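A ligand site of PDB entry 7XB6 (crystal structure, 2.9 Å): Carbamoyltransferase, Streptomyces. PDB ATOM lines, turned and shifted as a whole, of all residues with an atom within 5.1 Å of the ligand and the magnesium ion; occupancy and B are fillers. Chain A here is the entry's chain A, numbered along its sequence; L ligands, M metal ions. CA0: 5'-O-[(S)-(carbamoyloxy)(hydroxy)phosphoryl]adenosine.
Four residues have an atom within 4 Å of the magnesium ion: His 157, His 161, Asp 180 and Asp 363. The nearest printed residue that does not touch the magnesium ion is Val 366 (4.6 Å).
A nitrogen (N2B) of the ligand is bound to the magnesium ion, 1.8 Å away. OD1 of Asp 363 is bound to the magnesium ion (1.9 Å). OD2 of Asp 180 is bound to the magnesium ion, at 2.1 Å. A ring nitrogen (NE2) of His 157 binds the magnesium ion (2.1 Å). The magnesium ion is bound by NE2 of His 161 (2.2 Å). An oxygen (O2A) of the ligand binds the magnesium ion. The magnesium ion has six donor atoms within binding distance.
N of Asp 363 lies within hydrogen-bond range of O1A of the ligand, 3.4 Å away. OE2 of Glu 231 sits at hydrogen-bond distance from O2' of the ligand. ND2 of Asn 339 sits at hydrogen-bond distance from N1 of the ligand (2.8 Å). O3A of the ligand lies within hydrogen-bond range of NE2 of His 35, 3.1 Å away. The backbone NH (N) of Gly 335 sits close to an oxygen (O2A) of the ligand (3.5 Å). O of Ala 213 sits at hydrogen-bond distance from O3' of the ligand. N6 of the ligand is in hydrogen-bond range of O of Leu 338 (3.5 Å).
OD2 of Asp 363 lies within hydrogen-bond range of NE2 of His 35, 3.4 Å away. The backbone NH of Gln 182 lies within hydrogen-bond range of the side-chain carboxylate of Asp 180 (2.9 Å). A ring nitrogen (ND1) of His 161 lies within hydrogen-bond range of the backbone carbonyl oxygen (O) of Ala 361, 2.9 Å away. The side-chain carboxylate (OE1) of Glu 231 sits at hydrogen-bond distance from the backbone NH (N) of Asn 228 (2.5 Å). The side-chain sulfur (SD) of Met 235 sits close to the side-chain amide oxygen (OD1) of Asn 339 (3.7 Å). The side-chain sulfur (SD) of Met 235 is in hydrogen-bond range of the backbone NH (N) of Cys 340.
Gly 181 touches the ligand. O of Gln 182 touches O1B of the ligand (3.5 Å). Gln 214 touches the ligand (N to O3', 3.9 Å). Phe 216 touches the ligand. CB of Ala 217 touches O2' of the ligand, 3.7 Å away. Asn 228 touches the ligand. Met 235 touches the ligand (CE to N6, 3.2 Å). Leu 336 touches the ligand. Ser 362 touches the ligand. Hydrophobic or aromatic side chains within 4 Å of the ligand: His 35, His 157, His 161, Ala 213, Phe 216, Ala 217, Met 235, Leu 336 and Leu 338. The nearest printed residue that does not touch the ligand is Gly 334 (4.4 Å).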
ATOM      1  N   HIS A  35      33.058 -26.188  22.635  1.00  0.00           N
ATOM      2  CA  HIS A  35      34.099 -26.972  21.916  1.00  0.00           C
ATOM      3  C   HIS A  35      34.719 -26.085  20.841  1.00  0.00           C
ATOM      4  O   HIS A  35      33.990 -25.243  20.279  1.00  0.00           O
ATOM      5  CB  HIS A  35      33.562 -28.294  21.343  1.00  0.00           C
ATOM      6  CG  HIS A  35      32.561 -28.137  20.242  1.00  0.00           C
ATOM      7  ND1 HIS A  35      31.217 -28.417  20.407  1.00  0.00           N
ATOM      8  CD2 HIS A  35      32.704 -27.746  18.961  1.00  0.00           C
ATOM      9  CE1 HIS A  35      30.575 -28.204  19.274  1.00  0.00           C
ATOM     10  NE2 HIS A  35      31.466 -27.778  18.373  1.00  0.00           N
ATOM     11  N   TRP A  91      28.497 -16.450  21.042  1.00  0.00           N
ATOM     12  CA  TRP A  91      27.203 -16.964  21.549  1.00  0.00           C
ATOM     13  C   TRP A  91      26.456 -15.769  22.100  1.00  0.00           C
ATOM     14  O   TRP A  91      27.118 -14.827  22.564  1.00  0.00           O
ATOM     15  CB  TRP A  91      27.399 -18.006  22.660  1.00  0.00           C
ATOM     16  CG  TRP A  91      28.117 -19.245  22.234  1.00  0.00           C
ATOM     17  CD1 TRP A  91      29.453 -19.497  22.345  1.00  0.00           C
ATOM     18  CD2 TRP A  91      27.540 -20.412  21.621  1.00  0.00           C
ATOM     19  NE1 TRP A  91      29.742 -20.738  21.851  1.00  0.00           N
ATOM     20  CE2 TRP A  91      28.587 -21.320  21.394  1.00  0.00           C
ATOM     21  CE3 TRP A  91      26.233 -20.767  21.240  1.00  0.00           C
ATOM     22  CZ2 TRP A  91      28.383 -22.565  20.800  1.00  0.00           C
ATOM     23  CZ3 TRP A  91      26.031 -21.999  20.652  1.00  0.00           C
ATOM     24  CH2 TRP A  91      27.088 -22.878  20.443  1.00  0.00           C
ATOM     25  N   HIS A 157      25.299 -16.945  17.660  1.00  0.00           N
ATOM     26  CA  HIS A 157      26.145 -18.051  17.144  1.00  0.00           C
ATOM     27  C   HIS A 157      26.071 -18.155  15.616  1.00  0.00           C
ATOM     28  O   HIS A 157      27.105 -18.074  14.967  1.00  0.00           O
ATOM     29  CB  HIS A 157      25.778 -19.368  17.836  1.00  0.00           C
ATOM     30  CG  HIS A 157      26.730 -20.455  17.479  1.00  0.00           C
ATOM     31  ND1 HIS A 157      27.836 -20.730  18.234  1.00  0.00           N
ATOM     32  CD2 HIS A 157      26.769 -21.299  16.418  1.00  0.00           C
ATOM     33  CE1 HIS A 157      28.500 -21.729  17.686  1.00  0.00           C
ATOM     34  NE2 HIS A 157      27.857 -22.092  16.570  1.00  0.00           N
ATOM     35  N   HIS A 161      29.112 -17.576  12.602  1.00  0.00           N
ATOM     36  CA  HIS A 161      29.372 -18.427  11.406  1.00  0.00           C
ATOM     37  C   HIS A 161      29.279 -17.566  10.149  1.00  0.00           C
ATOM     38  O   HIS A 161      30.212 -17.595   9.317  1.00  0.00           O
ATOM     39  CB  HIS A 161      28.378 -19.600  11.329  1.00  0.00           C
ATOM     40  CG  HIS A 161      28.672 -20.719  12.252  1.00  0.00           C
ATOM     41  ND1 HIS A 161      29.744 -21.565  12.055  1.00  0.00           N
ATOM     42  CD2 HIS A 161      28.022 -21.154  13.353  1.00  0.00           C
ATOM     43  CE1 HIS A 161      29.763 -22.468  13.023  1.00  0.00           C
ATOM     44  NE2 HIS A 161      28.714 -22.242  13.828  1.00  0.00           N
ATOM     45  N   ASP A 180      24.212 -25.733  11.556  1.00  0.00           N
ATOM     46  CA  ASP A 180      25.143 -26.288  12.574  1.00  0.00           C
ATOM     47  C   ASP A 180      24.367 -27.204  13.514  1.00  0.00           C
ATOM     48  O   ASP A 180      23.153 -27.339  13.331  1.00  0.00           O
ATOM     49  CB  ASP A 180      25.952 -25.182  13.280  1.00  0.00           C
ATOM     50  CG  ASP A 180      25.426 -24.645  14.591  1.00  0.00           C
ATOM     51  OD1 ASP A 180      24.269 -24.952  14.942  1.00  0.00           O
ATOM     52  OD2 ASP A 180      26.185 -23.912  15.239  1.00  0.00           O
ATOM     53  N   GLY A 181      25.065 -27.821  14.454  1.00  0.00           N
ATOM     54  CA  GLY A 181      24.409 -28.756  15.385  1.00  0.00           C
ATOM     55  C   GLY A 181      23.438 -28.068  16.302  1.00  0.00           C
ATOM     56  O   GLY A 181      22.274 -28.506  16.369  1.00  0.00           O
ATOM     57  N   GLN A 182      23.868 -27.013  16.981  1.00  0.00           N
ATOM     58  CA  GLN A 182      22.891 -26.272  17.813  1.00  0.00           C
ATOM     59  C   GLN A 182      23.366 -24.858  18.124  1.00  0.00           C
ATOM     60  O   GLN A 182      24.547 -24.694  18.481  1.00  0.00           O
ATOM     61  CB  GLN A 182      22.638 -27.007  19.131  1.00  0.00           C
ATOM     62  CG  GLN A 182      21.711 -26.249  20.070  1.00  0.00           C
ATOM     63  CD  GLN A 182      21.210 -27.100  21.209  1.00  0.00           C
ATOM     64  OE1 GLN A 182      21.379 -28.311  21.228  1.00  0.00           O
ATOM     65  NE2 GLN A 182      20.569 -26.452  22.176  1.00  0.00           N
ATOM     66  N   ALA A 213      22.227 -31.665  11.723  1.00  0.00           N
ATOM     67  CA  ALA A 213      23.645 -31.877  12.074  1.00  0.00           C
ATOM     68  C   ALA A 213      23.751 -32.893  13.222  1.00  0.00           C
ATOM     69  O   ALA A 213      24.624 -33.792  13.146  1.00  0.00           O
ATOM     70  CB  ALA A 213      24.250 -30.559  12.443  1.00  0.00           C
ATOM     71  N   GLN A 214      22.895 -32.756  14.228  1.00  0.00           N
ATOM     72  CA  GLN A 214      22.890 -33.629  15.434  1.00  0.00           C
ATOM     73  C   GLN A 214      22.304 -35.012  15.102  1.00  0.00           C
ATOM     74  O   GLN A 214      22.598 -35.986  15.837  1.00  0.00           O
ATOM     75  CB  GLN A 214      22.125 -32.912  16.546  1.00  0.00           C
ATOM     76  CG  GLN A 214      22.353 -33.483  17.937  1.00  0.00           C
ATOM     77  CD  GLN A 214      21.328 -32.951  18.906  1.00  0.00           C
ATOM     78  OE1 GLN A 214      20.871 -33.654  19.802  1.00  0.00           O
ATOM     79  NE2 GLN A 214      20.964 -31.681  18.718  1.00  0.00           N
ATOM     80  N   PHE A 216      23.047 -36.594  12.146  1.00  0.00           N
ATOM     81  CA  PHE A 216      24.324 -37.171  11.653  1.00  0.00           C
ATOM     82  C   PHE A 216      25.184 -37.545  12.861  1.00  0.00           C
ATOM     83  O   PHE A 216      25.746 -38.668  12.888  1.00  0.00           O
ATOM     84  CB  PHE A 216      25.008 -36.215  10.684  1.00  0.00           C
ATOM     85  CG  PHE A 216      25.975 -36.898   9.738  1.00  0.00           C
ATOM     86  CD1 PHE A 216      25.515 -37.501   8.571  1.00  0.00           C
ATOM     87  CD2 PHE A 216      27.333 -36.947  10.018  1.00  0.00           C
ATOM     88  CE1 PHE A 216      26.393 -38.128   7.701  1.00  0.00           C
ATOM     89  CE2 PHE A 216      28.211 -37.575   9.149  1.00  0.00           C
ATOM     90  CZ  PHE A 216      27.746 -38.168   7.994  1.00  0.00           C
ATOM     91  N   ALA A 217      25.265 -36.659  13.863  1.00  0.00           N
ATOM     92  CA  ALA A 217      26.039 -36.891  15.110  1.00  0.00           C
ATOM     93  C   ALA A 217      25.557 -38.151  15.827  1.00  0.00           C
ATOM     94  O   ALA A 217      26.406 -38.990  16.206  1.00  0.00           O
ATOM     95  CB  ALA A 217      25.955 -35.684  16.013  1.00  0.00           C
ATOM     96  N   ASN A 228      30.718 -35.542  17.003  1.00  0.00           N
ATOM     97  CA  ASN A 228      31.290 -34.187  17.174  1.00  0.00           C
ATOM     98  C   ASN A 228      32.811 -34.249  17.154  1.00  0.00           C
ATOM     99  O   ASN A 228      33.426 -33.234  17.502  1.00  0.00           O
ATOM    100  CB  ASN A 228      30.697 -33.490  18.407  1.00  0.00           C
ATOM    101  CG  ASN A 228      29.204 -33.304  18.314  1.00  0.00           C
ATOM    102  OD1 ASN A 228      28.733 -32.243  17.891  1.00  0.00           O
ATOM    103  ND2 ASN A 228      28.452 -34.317  18.688  1.00  0.00           N
ATOM    104  N   GLU A 231      32.751 -37.442  12.555  1.00  0.00           N
ATOM    105  CA  GLU A 231      31.631 -37.543  11.580  1.00  0.00           C
ATOM    106  C   GLU A 231      32.151 -37.857  10.186  1.00  0.00           C
ATOM    107  O   GLU A 231      31.395 -38.416   9.389  1.00  0.00           O
ATOM    108  CB  GLU A 231      30.871 -36.216  11.552  1.00  0.00           C
ATOM    109  CG  GLU A 231      31.205 -35.305  12.709  1.00  0.00           C
ATOM    110  CD  GLU A 231      30.830 -35.860  14.073  1.00  0.00           C
ATOM    111  OE1 GLU A 231      31.759 -36.225  14.820  1.00  0.00           O
ATOM    112  OE2 GLU A 231      29.633 -35.922  14.374  1.00  0.00           O
ATOM    113  N   TYR A 232      33.402 -37.494   9.895  1.00  0.00           N
ATOM    114  CA  TYR A 232      34.016 -37.706   8.563  1.00  0.00           C
ATOM    115  C   TYR A 232      34.134 -39.205   8.315  1.00  0.00           C
ATOM    116  O   TYR A 232      34.209 -39.626   7.148  1.00  0.00           O
ATOM    117  CB  TYR A 232      35.407 -37.086   8.566  1.00  0.00           C
ATOM    118  CG  TYR A 232      36.358 -37.666   9.580  1.00  0.00           C
ATOM    119  CD1 TYR A 232      36.397 -37.181  10.871  1.00  0.00           C
ATOM    120  CD2 TYR A 232      37.206 -38.702   9.242  1.00  0.00           C
ATOM    121  CE1 TYR A 232      37.259 -37.715  11.806  1.00  0.00           C
ATOM    122  CE2 TYR A 232      38.085 -39.239  10.164  1.00  0.00           C
ATOM    123  CZ  TYR A 232      38.103 -38.744  11.452  1.00  0.00           C
ATOM    124  OH  TYR A 232      38.965 -39.279  12.373  1.00  0.00           O
ATOM    125  N   MET A 235      30.901 -40.007   6.520  1.00  0.00           N
ATOM    126  CA  MET A 235      31.139 -39.479   5.147  1.00  0.00           C
ATOM    127  C   MET A 235      32.100 -40.418   4.416  1.00  0.00           C
ATOM    128  O   MET A 235      31.806 -40.844   3.275  1.00  0.00           O
ATOM    129  CB  MET A 235      31.732 -38.064   5.177  1.00  0.00           C
ATOM    130  CG  MET A 235      31.463 -37.297   3.897  1.00  0.00           C
ATOM    131  SD  MET A 235      32.554 -35.884   3.614  1.00  0.00           S
ATOM    132  CE  MET A 235      33.054 -35.486   5.291  1.00  0.00           C
ATOM    133  N   ILE A 310      21.639 -36.055   4.536  1.00  0.00           N
ATOM    134  CA  ILE A 310      22.453 -34.800   4.476  1.00  0.00           C
ATOM    135  C   ILE A 310      22.247 -34.147   3.105  1.00  0.00           C
ATOM    136  O   ILE A 310      21.829 -32.963   3.075  1.00  0.00           O
ATOM    137  CB  ILE A 310      23.940 -35.088   4.767  1.00  0.00           C
ATOM    138  CG1 ILE A 310      24.164 -35.586   6.206  1.00  0.00           C
ATOM    139  CG2 ILE A 310      24.817 -33.880   4.444  1.00  0.00           C
ATOM    140  CD1 ILE A 310      23.475 -34.757   7.271  1.00  0.00           C
ATOM    141  N   GLY A 334      28.768 -23.213   9.079  1.00  0.00           N
ATOM    142  CA  GLY A 334      28.257 -24.130  10.104  1.00  0.00           C
ATOM    143  C   GLY A 334      28.804 -25.522   9.863  1.00  0.00           C
ATOM    144  O   GLY A 334      29.343 -25.774   8.783  1.00  0.00           O
ATOM    145  N   GLY A 335      28.603 -26.415  10.816  1.00  0.00           N
ATOM    146  CA  GLY A 335      29.309 -27.695  10.894  1.00  0.00           C
ATOM    147  C   GLY A 335      28.894 -28.691   9.831  1.00  0.00           C
ATOM    148  O   GLY A 335      29.644 -29.637   9.614  1.00  0.00           O
ATOM    149  N   LEU A 336      27.728 -28.540   9.231  1.00  0.00           N
ATOM    150  CA  LEU A 336      27.296 -29.489   8.168  1.00  0.00           C
ATOM    151  C   LEU A 336      28.045 -29.165   6.870  1.00  0.00           C
ATOM    152  O   LEU A 336      28.031 -30.038   5.960  1.00  0.00           O
ATOM    153  CB  LEU A 336      25.797 -29.389   7.957  1.00  0.00           C
ATOM    154  CG  LEU A 336      25.167 -30.680   7.463  1.00  0.00           C
ATOM    155  CD1 LEU A 336      24.545 -31.433   8.622  1.00  0.00           C
ATOM    156  CD2 LEU A 336      24.164 -30.411   6.355  1.00  0.00           C
ATOM    157  N   LEU A 338      31.094 -29.061   6.911  1.00  0.00           N
ATOM    158  CA  LEU A 338      32.251 -29.975   7.072  1.00  0.00           C
ATOM    159  C   LEU A 338      32.099 -31.200   6.172  1.00  0.00           C
ATOM    160  O   LEU A 338      33.105 -31.896   6.004  1.00  0.00           O
ATOM    161  CB  LEU A 338      32.393 -30.433   8.533  1.00  0.00           C
ATOM    162  CG  LEU A 338      33.097 -29.494   9.505  1.00  0.00           C
ATOM    163  CD1 LEU A 338      33.494 -30.218  10.791  1.00  0.00           C
ATOM    164  CD2 LEU A 338      34.334 -28.843   8.881  1.00  0.00           C
ATOM    165  N   ASN A 339      30.901 -31.495   5.659  1.00  0.00           N
ATOM    166  CA  ASN A 339      30.664 -32.633   4.724  1.00  0.00           C
ATOM    167  C   ASN A 339      31.083 -32.197   3.317  1.00  0.00           C
ATOM    168  O   ASN A 339      30.216 -31.721   2.567  1.00  0.00           O
ATOM    169  CB  ASN A 339      29.209 -33.126   4.732  1.00  0.00           C
ATOM    170  CG  ASN A 339      29.070 -34.541   4.224  1.00  0.00           C
ATOM    171  OD1 ASN A 339      29.061 -34.784   3.013  1.00  0.00           O
ATOM    172  ND2 ASN A 339      28.949 -35.500   5.131  1.00  0.00           N
ATOM    173  N   CYS A 340      32.367 -32.341   3.001  1.00  0.00           N
ATOM    174  CA  CYS A 340      32.985 -31.756   1.782  1.00  0.00           C
ATOM    175  C   CYS A 340      32.398 -32.456   0.551  1.00  0.00           C
ATOM    176  O   CYS A 340      32.239 -31.780  -0.480  1.00  0.00           O
ATOM    177  CB  CYS A 340      34.527 -31.774   1.851  1.00  0.00           C
ATOM    178  SG  CYS A 340      35.280 -33.231   2.634  1.00  0.00           S
ATOM    179  N   ALA A 361      34.203 -23.054   8.961  1.00  0.00           N
ATOM    180  CA  ALA A 361      32.758 -23.307   8.863  1.00  0.00           C
ATOM    181  C   ALA A 361      32.290 -23.868  10.197  1.00  0.00           C
ATOM    182  O   ALA A 361      31.144 -23.635  10.571  1.00  0.00           O
ATOM    183  CB  ALA A 361      32.512 -24.281   7.752  1.00  0.00           C
ATOM    184  N   SER A 362      33.179 -24.581  10.862  1.00  0.00           N
ATOM    185  CA  SER A 362      32.845 -25.189  12.177  1.00  0.00           C
ATOM    186  C   SER A 362      32.927 -24.143  13.275  1.00  0.00           C
ATOM    187  O   SER A 362      33.167 -22.977  12.960  1.00  0.00           O
ATOM    188  CB  SER A 362      33.785 -26.328  12.416  1.00  0.00           C
ATOM    189  OG  SER A 362      35.025 -26.121  11.758  1.00  0.00           O
ATOM    190  N   ASP A 363      32.749 -24.579  14.510  1.00  0.00           N
ATOM    191  CA  ASP A 363      32.708 -23.616  15.636  1.00  0.00           C
ATOM    192  C   ASP A 363      34.056 -22.916  15.807  1.00  0.00           C
ATOM    193  O   ASP A 363      34.050 -21.782  16.286  1.00  0.00           O
ATOM    194  CB  ASP A 363      32.140 -24.283  16.887  1.00  0.00           C
ATOM    195  CG  ASP A 363      30.630 -24.336  16.935  1.00  0.00           C
ATOM    196  OD1 ASP A 363      29.994 -24.003  15.916  1.00  0.00           O
ATOM    197  OD2 ASP A 363      30.098 -24.694  17.987  1.00  0.00           O
ATOM    198  N   VAL A 366      33.829 -19.386  14.738  1.00  0.00           N
ATOM    199  CA  VAL A 366      32.853 -18.424  15.353  1.00  0.00           C
ATOM    200  C   VAL A 366      33.625 -17.409  16.203  1.00  0.00           C
ATOM    201  O   VAL A 366      33.038 -16.356  16.519  1.00  0.00           O
ATOM    202  CB  VAL A 366      31.716 -19.090  16.160  1.00  0.00           C
ATOM    203  CG1 VAL A 366      30.969 -20.124  15.326  1.00  0.00           C
ATOM    204  CG2 VAL A 366      32.172 -19.677  17.488  1.00  0.00           C
HETATM  205  N1  CA0 L   1      28.747 -34.170   7.605  1.00  0.00           N
HETATM  206  C2  CA0 L   1      27.682 -33.825   8.338  1.00  0.00           C
HETATM  207  N3  CA0 L   1      27.624 -33.308   9.565  1.00  0.00           N
HETATM  208  C4  CA0 L   1      28.866 -33.131  10.050  1.00  0.00           C
HETATM  209  C5  CA0 L   1      30.054 -33.431   9.429  1.00  0.00           C
HETATM  210  C6  CA0 L   1      29.977 -33.970   8.130  1.00  0.00           C
HETATM  211  N6  CA0 L   1      31.047 -34.309   7.417  1.00  0.00           N
HETATM  212  N7  CA0 L   1      31.119 -33.107  10.248  1.00  0.00           N
HETATM  213  C8  CA0 L   1      30.571 -32.633  11.338  1.00  0.00           C
HETATM  214  N9  CA0 L   1      29.203 -32.627  11.283  1.00  0.00           N
HETATM  215  PA  CA0 L   1      29.414 -26.948  15.033  1.00  0.00           P
HETATM  216  CB  CA0 L   1      27.993 -26.228  17.080  1.00  0.00           C
HETATM  217  C1' CA0 L   1      28.275 -32.175  12.300  1.00  0.00           C
HETATM  218  O1A CA0 L   1      30.831 -27.319  14.790  1.00  0.00           O
HETATM  219  O1B CA0 L   1      27.267 -26.815  17.840  1.00  0.00           O
HETATM  220  C2' CA0 L   1      28.767 -32.403  13.723  1.00  0.00           C
HETATM  221  O2' CA0 L   1      28.522 -33.725  14.163  1.00  0.00           O
HETATM  222  O2A CA0 L   1      28.820 -25.856  14.218  1.00  0.00           O
HETATM  223  N2B CA0 L   1      27.776 -24.999  16.609  1.00  0.00           N
HETATM  224  C3' CA0 L   1      27.966 -31.355  14.482  1.00  0.00           C
HETATM  225  O3' CA0 L   1      26.659 -31.826  14.770  1.00  0.00           O
HETATM  226  O3A CA0 L   1      29.141 -26.722  16.608  1.00  0.00           O
HETATM  227  C4' CA0 L   1      27.922 -30.187  13.482  1.00  0.00           C
HETATM  228  O4' CA0 L   1      28.124 -30.787  12.176  1.00  0.00           O
HETATM  229  C5' CA0 L   1      28.961 -29.110  13.678  1.00  0.00           C
HETATM  230  O5' CA0 L   1      28.553 -28.269  14.778  1.00  0.00           O
HETATM  231 MG    MG M   1      28.239 -23.767  15.325  1.00  0.00          MG
